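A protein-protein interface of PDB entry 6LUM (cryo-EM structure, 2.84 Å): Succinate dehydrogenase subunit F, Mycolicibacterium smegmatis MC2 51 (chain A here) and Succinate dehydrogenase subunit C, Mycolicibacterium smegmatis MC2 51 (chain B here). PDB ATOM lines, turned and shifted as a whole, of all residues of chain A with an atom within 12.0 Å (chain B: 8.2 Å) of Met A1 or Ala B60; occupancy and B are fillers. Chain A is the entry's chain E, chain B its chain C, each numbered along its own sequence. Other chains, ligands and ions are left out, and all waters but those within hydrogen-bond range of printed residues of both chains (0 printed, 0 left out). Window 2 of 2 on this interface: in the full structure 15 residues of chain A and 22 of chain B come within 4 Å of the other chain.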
ATOM      1  N   MET A   1     -17.682  24.168 -16.013  1.00  0.00           N
ATOM      2  CA  MET A   1     -16.262  24.464 -16.179  1.00  0.00           C
ATOM      3  C   MET A   1     -15.472  23.528 -15.291  1.00  0.00           C
ATOM      4  O   MET A   1     -14.648  22.760 -15.761  1.00  0.00           O
ATOM      5  CB  MET A   1     -15.971  25.928 -15.834  1.00  0.00           C
ATOM      6  CG  MET A   1     -14.582  26.479 -16.231  1.00  0.00           C
ATOM      7  SD  MET A   1     -13.108  25.442 -16.149  1.00  0.00           S
ATOM      8  CE  MET A   1     -12.338  26.103 -14.673  1.00  0.00           C
ATOM      9  N   VAL A   2     -15.731  23.607 -13.987  1.00  0.00           N
ATOM     10  CA  VAL A   2     -15.191  22.609 -13.072  1.00  0.00           C
ATOM     11  C   VAL A   2     -15.698  21.227 -13.459  1.00  0.00           C
ATOM     12  O   VAL A   2     -14.996  20.214 -13.310  1.00  0.00           O
ATOM     13  CB  VAL A   2     -15.563  22.980 -11.626  1.00  0.00           C
ATOM     14  CG1 VAL A   2     -15.733  21.743 -10.775  1.00  0.00           C
ATOM     15  CG2 VAL A   2     -14.523  23.890 -11.049  1.00  0.00           C
ATOM     16  N   LEU A   3     -16.920  21.172 -13.987  1.00  0.00           N
ATOM     17  CA  LEU A   3     -17.477  19.916 -14.459  1.00  0.00           C
ATOM     18  C   LEU A   3     -16.623  19.304 -15.554  1.00  0.00           C
ATOM     19  O   LEU A   3     -16.442  18.086 -15.583  1.00  0.00           O
ATOM     20  CB  LEU A   3     -18.900  20.130 -14.956  1.00  0.00           C
ATOM     21  CG  LEU A   3     -19.593  18.832 -15.351  1.00  0.00           C
ATOM     22  CD1 LEU A   3     -20.832  18.622 -14.512  1.00  0.00           C
ATOM     23  CD2 LEU A   3     -19.947  18.865 -16.813  1.00  0.00           C
ATOM     24  N   PHE A   4     -16.082  20.122 -16.455  1.00  0.00           N
ATOM     25  CA  PHE A   4     -15.201  19.589 -17.487  1.00  0.00           C
ATOM     26  C   PHE A   4     -13.999  18.886 -16.878  1.00  0.00           C
ATOM     27  O   PHE A   4     -13.595  17.820 -17.346  1.00  0.00           O
ATOM     28  CB  PHE A   4     -14.747  20.706 -18.418  1.00  0.00           C
ATOM     29  CG  PHE A   4     -13.624  20.320 -19.331  1.00  0.00           C
ATOM     30  CD1 PHE A   4     -13.709  19.203 -20.131  1.00  0.00           C
ATOM     31  CD2 PHE A   4     -12.481  21.086 -19.391  1.00  0.00           C
ATOM     32  CE1 PHE A   4     -12.672  18.859 -20.969  1.00  0.00           C
ATOM     33  CE2 PHE A   4     -11.444  20.746 -20.224  1.00  0.00           C
ATOM     34  CZ  PHE A   4     -11.538  19.631 -21.014  1.00  0.00           C
ATOM     35  N   PHE A   5     -13.443  19.437 -15.806  1.00  0.00           N
ATOM     36  CA  PHE A   5     -12.230  18.847 -15.266  1.00  0.00           C
ATOM     37  C   PHE A   5     -12.513  17.638 -14.396  1.00  0.00           C
ATOM     38  O   PHE A   5     -11.694  16.716 -14.353  1.00  0.00           O
ATOM     39  CB  PHE A   5     -11.430  19.901 -14.515  1.00  0.00           C
ATOM     40  CG  PHE A   5     -10.596  20.731 -15.419  1.00  0.00           C
ATOM     41  CD1 PHE A   5      -9.416  20.236 -15.921  1.00  0.00           C
ATOM     42  CD2 PHE A   5     -11.024  21.971 -15.833  1.00  0.00           C
ATOM     43  CE1 PHE A   5      -8.663  20.974 -16.778  1.00  0.00           C
ATOM     44  CE2 PHE A   5     -10.268  22.714 -16.695  1.00  0.00           C
ATOM     45  CZ  PHE A   5      -9.087  22.216 -17.167  1.00  0.00           C
ATOM     46  N   GLU A   6     -13.667  17.571 -13.737  1.00  0.00           N
ATOM     47  CA  GLU A   6     -13.991  16.322 -13.050  1.00  0.00           C
ATOM     48  C   GLU A   6     -14.345  15.226 -14.053  1.00  0.00           C
ATOM     49  O   GLU A   6     -14.032  14.050 -13.838  1.00  0.00           O
ATOM     50  CB  GLU A   6     -15.112  16.532 -12.040  1.00  0.00           C
ATOM     51  CG  GLU A   6     -16.355  17.145 -12.602  1.00  0.00           C
ATOM     52  CD  GLU A   6     -17.498  17.108 -11.620  1.00  0.00           C
ATOM     53  OE1 GLU A   6     -17.265  16.720 -10.457  1.00  0.00           O
ATOM     54  OE2 GLU A   6     -18.627  17.472 -12.007  1.00  0.00           O
ATOM     55  N   ILE A   7     -14.981  15.596 -15.169  1.00  0.00           N
ATOM     56  CA  ILE A   7     -15.193  14.641 -16.254  1.00  0.00           C
ATOM     57  C   ILE A   7     -13.859  14.133 -16.783  1.00  0.00           C
ATOM     58  O   ILE A   7     -13.684  12.933 -17.030  1.00  0.00           O
ATOM     59  CB  ILE A   7     -16.040  15.285 -17.367  1.00  0.00           C
ATOM     60  CG1 ILE A   7     -17.466  15.542 -16.866  1.00  0.00           C
ATOM     61  CG2 ILE A   7     -16.004  14.446 -18.631  1.00  0.00           C
ATOM     62  CD1 ILE A   7     -18.548  15.253 -17.863  1.00  0.00           C
ATOM     63  N   LEU A   8     -12.894  15.035 -16.955  1.00  0.00           N
ATOM     64  CA  LEU A   8     -11.560  14.631 -17.380  1.00  0.00           C
ATOM     65  C   LEU A   8     -10.919  13.690 -16.370  1.00  0.00           C
ATOM     66  O   LEU A   8     -10.243  12.732 -16.752  1.00  0.00           O
ATOM     67  CB  LEU A   8     -10.689  15.865 -17.586  1.00  0.00           C
ATOM     68  CG  LEU A   8      -9.646  15.755 -18.687  1.00  0.00           C
ATOM     69  CD1 LEU A   8     -10.312  15.372 -19.980  1.00  0.00           C
ATOM     70  CD2 LEU A   8      -8.908  17.063 -18.831  1.00  0.00           C
ATOM     71  N   LEU A   9     -11.118  13.949 -15.081  1.00  0.00           N
ATOM     72  CA  LEU A   9     -10.546  13.083 -14.057  1.00  0.00           C
ATOM     73  C   LEU A   9     -11.124  11.677 -14.128  1.00  0.00           C
ATOM     74  O   LEU A   9     -10.381  10.688 -14.058  1.00  0.00           O
ATOM     75  CB  LEU A   9     -10.784  13.687 -12.680  1.00  0.00           C
ATOM     76  CG  LEU A   9      -9.961  13.153 -11.514  1.00  0.00           C
ATOM     77  CD1 LEU A   9      -8.586  13.776 -11.515  1.00  0.00           C
ATOM     78  CD2 LEU A   9     -10.668  13.436 -10.206  1.00  0.00           C
ATOM     79  N   VAL A  10     -12.444  11.553 -14.264  1.00  0.00           N
ATOM     80  CA  VAL A  10     -13.007  10.205 -14.303  1.00  0.00           C
ATOM     81  C   VAL A  10     -12.616   9.504 -15.597  1.00  0.00           C
ATOM     82  O   VAL A  10     -12.402   8.289 -15.613  1.00  0.00           O
ATOM     83  CB  VAL A  10     -14.530  10.215 -14.104  1.00  0.00           C
ATOM     84  CG1 VAL A  10     -14.855  10.146 -12.628  1.00  0.00           C
ATOM     85  CG2 VAL A  10     -15.157  11.408 -14.741  1.00  0.00           C
ATOM     86  N   ASP B  50      -4.783  20.760 -16.252  1.00  0.00           N
ATOM     87  CA  ASP B  50      -5.349  21.541 -15.155  1.00  0.00           C
ATOM     88  C   ASP B  50      -4.376  22.571 -14.610  1.00  0.00           C
ATOM     89  O   ASP B  50      -4.805  23.512 -13.943  1.00  0.00           O
ATOM     90  CB  ASP B  50      -5.856  20.621 -14.037  1.00  0.00           C
ATOM     91  CG  ASP B  50      -4.752  20.065 -13.137  1.00  0.00           C
ATOM     92  OD1 ASP B  50      -3.731  20.724 -12.874  1.00  0.00           O
ATOM     93  OD2 ASP B  50      -4.917  18.924 -12.662  1.00  0.00           O
ATOM     94  N   LEU B  53      -4.443  25.690 -16.696  1.00  0.00           N
ATOM     95  CA  LEU B  53      -5.519  26.569 -16.249  1.00  0.00           C
ATOM     96  C   LEU B  53      -5.041  27.744 -15.404  1.00  0.00           C
ATOM     97  O   LEU B  53      -5.855  28.524 -14.914  1.00  0.00           O
ATOM     98  CB  LEU B  53      -6.531  25.762 -15.450  1.00  0.00           C
ATOM     99  CG  LEU B  53      -7.973  26.192 -15.530  1.00  0.00           C
ATOM    100  CD1 LEU B  53      -8.465  25.964 -16.921  1.00  0.00           C
ATOM    101  CD2 LEU B  53      -8.723  25.352 -14.577  1.00  0.00           C
ATOM    102  N   VAL B  54      -3.732  27.875 -15.197  1.00  0.00           N
ATOM    103  CA  VAL B  54      -3.209  28.955 -14.363  1.00  0.00           C
ATOM    104  C   VAL B  54      -2.957  30.206 -15.182  1.00  0.00           C
ATOM    105  O   VAL B  54      -2.630  31.256 -14.614  1.00  0.00           O
ATOM    106  CB  VAL B  54      -1.918  28.506 -13.649  1.00  0.00           C
ATOM    107  CG1 VAL B  54      -0.729  28.618 -14.559  1.00  0.00           C
ATOM    108  CG2 VAL B  54      -1.709  29.242 -12.369  1.00  0.00           C
ATOM    109  N   ARG B  55      -3.105  30.127 -16.501  1.00  0.00           N
ATOM    110  CA  ARG B  55      -2.923  31.247 -17.407  1.00  0.00           C
ATOM    111  C   ARG B  55      -4.236  31.887 -17.822  1.00  0.00           C
ATOM    112  O   ARG B  55      -4.233  32.766 -18.681  1.00  0.00           O
ATOM    113  CB  ARG B  55      -2.163  30.797 -18.652  1.00  0.00           C
ATOM    114  CG  ARG B  55      -0.685  30.620 -18.455  1.00  0.00           C
ATOM    115  CD  ARG B  55       0.025  31.935 -18.399  1.00  0.00           C
ATOM    116  NE  ARG B  55       0.033  32.603 -19.687  1.00  0.00           N
ATOM    117  CZ  ARG B  55      -0.372  33.850 -19.873  1.00  0.00           C
ATOM    118  NH1 ARG B  55      -0.815  34.557 -18.853  1.00  0.00           N
ATOM    119  NH2 ARG B  55      -0.340  34.390 -21.077  1.00  0.00           N
ATOM    120  N   VAL B  56      -5.358  31.476 -17.243  1.00  0.00           N
ATOM    121  CA  VAL B  56      -6.637  32.093 -17.543  1.00  0.00           C
ATOM    122  C   VAL B  56      -7.106  32.992 -16.406  1.00  0.00           C
ATOM    123  O   VAL B  56      -7.601  34.089 -16.654  1.00  0.00           O
ATOM    124  CB  VAL B  56      -7.697  31.025 -17.893  1.00  0.00           C
ATOM    125  CG1 VAL B  56      -7.183  30.115 -18.980  1.00  0.00           C
ATOM    126  CG2 VAL B  56      -8.121  30.232 -16.693  1.00  0.00           C
ATOM    127  N   SER B  57      -6.926  32.570 -15.157  1.00  0.00           N
ATOM    128  CA  SER B  57      -7.334  33.361 -14.008  1.00  0.00           C
ATOM    129  C   SER B  57      -6.889  32.690 -12.719  1.00  0.00           C
ATOM    130  O   SER B  57      -6.610  31.489 -12.710  1.00  0.00           O
ATOM    131  CB  SER B  57      -8.848  33.553 -13.984  1.00  0.00           C
ATOM    132  OG  SER B  57      -9.508  32.305 -14.020  1.00  0.00           O
ATOM    133  N   PRO B  58      -6.795  33.432 -11.617  1.00  0.00           N
ATOM    134  CA  PRO B  58      -6.622  32.770 -10.320  1.00  0.00           C
ATOM    135  C   PRO B  58      -7.830  31.967  -9.894  1.00  0.00           C
ATOM    136  O   PRO B  58      -7.674  30.897  -9.297  1.00  0.00           O
ATOM    137  CB  PRO B  58      -6.365  33.940  -9.365  1.00  0.00           C
ATOM    138  CG  PRO B  58      -5.897  35.038 -10.225  1.00  0.00           C
ATOM    139  CD  PRO B  58      -6.587  34.881 -11.525  1.00  0.00           C
ATOM    140  N   GLN B  59      -9.035  32.452 -10.187  1.00  0.00           N
ATOM    141  CA  GLN B  59     -10.237  31.832  -9.641  1.00  0.00           C
ATOM    142  C   GLN B  59     -10.521  30.479 -10.276  1.00  0.00           C
ATOM    143  O   GLN B  59     -10.987  29.565  -9.596  1.00  0.00           O
ATOM    144  CB  GLN B  59     -11.431  32.761  -9.814  1.00  0.00           C
ATOM    145  CG  GLN B  59     -11.187  34.165  -9.315  1.00  0.00           C
ATOM    146  CD  GLN B  59     -10.700  35.086 -10.411  1.00  0.00           C
ATOM    147  OE1 GLN B  59     -10.716  34.731 -11.586  1.00  0.00           O
ATOM    148  NE2 GLN B  59     -10.260  36.277 -10.029  1.00  0.00           N
ATOM    149  N   ALA B  60     -10.254  30.324 -11.571  1.00  0.00           N
ATOM    150  CA  ALA B  60     -10.475  29.032 -12.211  1.00  0.00           C
ATOM    151  C   ALA B  60      -9.538  27.974 -11.647  1.00  0.00           C
ATOM    152  O   ALA B  60      -9.954  26.843 -11.351  1.00  0.00           O
ATOM    153  CB  ALA B  60     -10.288  29.160 -13.717  1.00  0.00           C
ATOM    154  N   TYR B  61      -8.263  28.326 -11.497  1.00  0.00           N
ATOM    155  CA  TYR B  61      -7.307  27.405 -10.905  1.00  0.00           C
ATOM    156  C   TYR B  61      -7.718  27.042  -9.491  1.00  0.00           C
ATOM    157  O   TYR B  61      -7.723  25.864  -9.113  1.00  0.00           O
ATOM    158  CB  TYR B  61      -5.916  28.023 -10.913  1.00  0.00           C
ATOM    159  CG  TYR B  61      -4.841  27.051 -10.531  1.00  0.00           C
ATOM    160  CD1 TYR B  61      -4.517  26.001 -11.356  1.00  0.00           C
ATOM    161  CD2 TYR B  61      -4.161  27.174  -9.341  1.00  0.00           C
ATOM    162  CE1 TYR B  61      -3.550  25.115 -11.013  1.00  0.00           C
ATOM    163  CE2 TYR B  61      -3.192  26.285  -8.992  1.00  0.00           C
ATOM    164  CZ  TYR B  61      -2.890  25.259  -9.833  1.00  0.00           C
ATOM    165  OH  TYR B  61      -1.921  24.357  -9.503  1.00  0.00           O
ATOM    166  N   ASN B  62      -8.065  28.049  -8.692  1.00  0.00           N
ATOM    167  CA  ASN B  62      -8.483  27.785  -7.327  1.00  0.00           C
ATOM    168  C   ASN B  62      -9.684  26.859  -7.293  1.00  0.00           C
ATOM    169  O   ASN B  62      -9.735  25.942  -6.475  1.00  0.00           O
ATOM    170  CB  ASN B  62      -8.789  29.094  -6.614  1.00  0.00           C
ATOM    171  CG  ASN B  62      -7.550  29.865  -6.272  1.00  0.00           C
ATOM    172  OD1 ASN B  62      -6.458  29.509  -6.683  1.00  0.00           O
ATOM    173  ND2 ASN B  62      -7.710  30.933  -5.514  1.00  0.00           N
ATOM    174  N   GLU B  63     -10.646  27.058  -8.194  1.00  0.00           N
ATOM    175  CA  GLU B  63     -11.809  26.180  -8.247  1.00  0.00           C
ATOM    176  C   GLU B  63     -11.404  24.731  -8.462  1.00  0.00           C
ATOM    177  O   GLU B  63     -11.749  23.846  -7.664  1.00  0.00           O
ATOM    178  CB  GLU B  63     -12.742  26.617  -9.368  1.00  0.00           C
ATOM    179  CG  GLU B  63     -13.615  27.800  -9.057  1.00  0.00           C
ATOM    180  CD  GLU B  63     -14.461  28.190 -10.250  1.00  0.00           C
ATOM    181  OE1 GLU B  63     -14.495  27.408 -11.221  1.00  0.00           O
ATOM    182  OE2 GLU B  63     -15.081  29.272 -10.224  1.00  0.00           O
ATOM    183  N   VAL B  64     -10.687  24.460  -9.552  1.00  0.00           N
ATOM    184  CA  VAL B  64     -10.447  23.062  -9.897  1.00  0.00           C
ATOM    185  C   VAL B  64      -9.571  22.388  -8.848  1.00  0.00           C
ATOM    186  O   VAL B  64      -9.765  21.208  -8.526  1.00  0.00           O
ATOM    187  CB  VAL B  64      -9.864  22.934 -11.313  1.00  0.00           C
ATOM    188  CG1 VAL B  64     -10.704  23.729 -12.274  1.00  0.00           C
ATOM    189  CG2 VAL B  64      -8.429  23.377 -11.356  1.00  0.00           C
ATOM    190  N   ILE B  65      -8.632  23.121  -8.251  1.00  0.00           N
ATOM    191  CA  ILE B  65      -7.823  22.437  -7.250  1.00  0.00           C
ATOM    192  C   ILE B  65      -8.578  22.286  -5.941  1.00  0.00           C
ATOM    193  O   ILE B  65      -8.331  21.337  -5.195  1.00  0.00           O
ATOM    194  CB  ILE B  65      -6.479  23.136  -7.039  1.00  0.00           C
ATOM    195  CG1 ILE B  65      -6.694  24.518  -6.471  1.00  0.00           C
ATOM    196  CG2 ILE B  65      -5.720  23.194  -8.327  1.00  0.00           C
ATOM    197  CD1 ILE B  65      -5.439  25.174  -6.179  1.00  0.00           C
ATOM    198  N   GLU B  66      -9.508  23.189  -5.626  1.00  0.00           N
ATOM    199  CA  GLU B  66     -10.354  22.953  -4.462  1.00  0.00           C
ATOM    200  C   GLU B  66     -11.186  21.705  -4.662  1.00  0.00           C
ATOM    201  O   GLU B  66     -11.544  21.028  -3.695  1.00  0.00           O
ATOM    202  CB  GLU B  66     -11.257  24.153  -4.184  1.00  0.00           C
ATOM    203  CG  GLU B  66     -10.541  25.406  -3.699  1.00  0.00           C
ATOM    204  CD  GLU B  66      -9.970  25.279  -2.307  1.00  0.00           C
ATOM    205  OE1 GLU B  66     -10.588  24.605  -1.460  1.00  0.00           O
ATOM    206  OE2 GLU B  66      -8.891  25.857  -2.063  1.00  0.00           O
ATOM    207  N   THR B  67     -11.512  21.383  -5.912  1.00  0.00           N
ATOM    208  CA  THR B  67     -12.179  20.105  -6.152  1.00  0.00           C
ATOM    209  C   THR B  67     -11.181  18.952  -6.171  1.00  0.00           C
ATOM    210  O   THR B  67     -11.579  17.785  -6.159  1.00  0.00           O
ATOM    211  CB  THR B  67     -12.984  20.125  -7.453  1.00  0.00           C
ATOM    212  OG1 THR B  67     -12.110  19.923  -8.566  1.00  0.00           O
ATOM    213  CG2 THR B  67     -13.731  21.441  -7.608  1.00  0.00           C
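OG1 of Thr B67 sits at hydrogen-bond distance from O of Val B64 (2.7 Å).
The side-chain hydroxyl (OG) of Ser B57 is in hydrogen-bond range of the backbone NH (N) of Ala B60 (3.2 Å).
Among the printed residues, merely in contact across the chains: Met A1 with Leu B53 (3.7 Å), Met A1 with Ala B60 (3.8 Å), Met A1 with Val B64 (3.7 Å), Val A2 with Glu B63 (3.5 Å), Val A2 with Thr B67 (3.8 Å), Phe A5 with Asp B50 (3.7 Å), Phe A5 with Leu B53 (3.7 Å) and Phe A5 with Val B64 (3.98 Å).
Of chain A, only Met A1 comes within 4 Å of Ala B60.
Of the printed residues of chain A, Leu B53 touches Met A1 (3.7 Å) and Phe A5 (3.7 Å).
No residue of chain A comes within 4 Å of Val B56.
No residue of chain A comes within 4 Å of Pro B58.
Gln B59 touches none of the printed residues of chain A.
No residue of chain A comes within 4 Å of Asn B62.
Printed residues of chain A within 4 Å of Asp B50: Phe A5 (3.7 Å).
Printed residues of chain B within 4 Å of Phe A5: Asp B50 (3.7 Å), Leu B53 (3.7 Å) and Val B64 (3.98 Å).
Printed residues of chain A within 4 Å of Val B64: Met A1 (3.7 Å) and Phe A5 (3.98 Å).
Of the printed residues of chain A, Thr B67 touches Val A2.
Ile A7 touches none of the printed residues of chain B.
Phe A4 touches none of the printed residues of chain B.
The nearest residue of chain B that does not touch Met A1 is Glu B63 (4.3 Å).
Of the 16 printed residues of chain B, 6 touch a printed residue of chain A.
Hydrophobic or aromatic side chains of chain A that line the printed part of chain B: Met A1, Val A2 and Phe A5.
Among the printed residues, 8 pairs touch across the chains.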
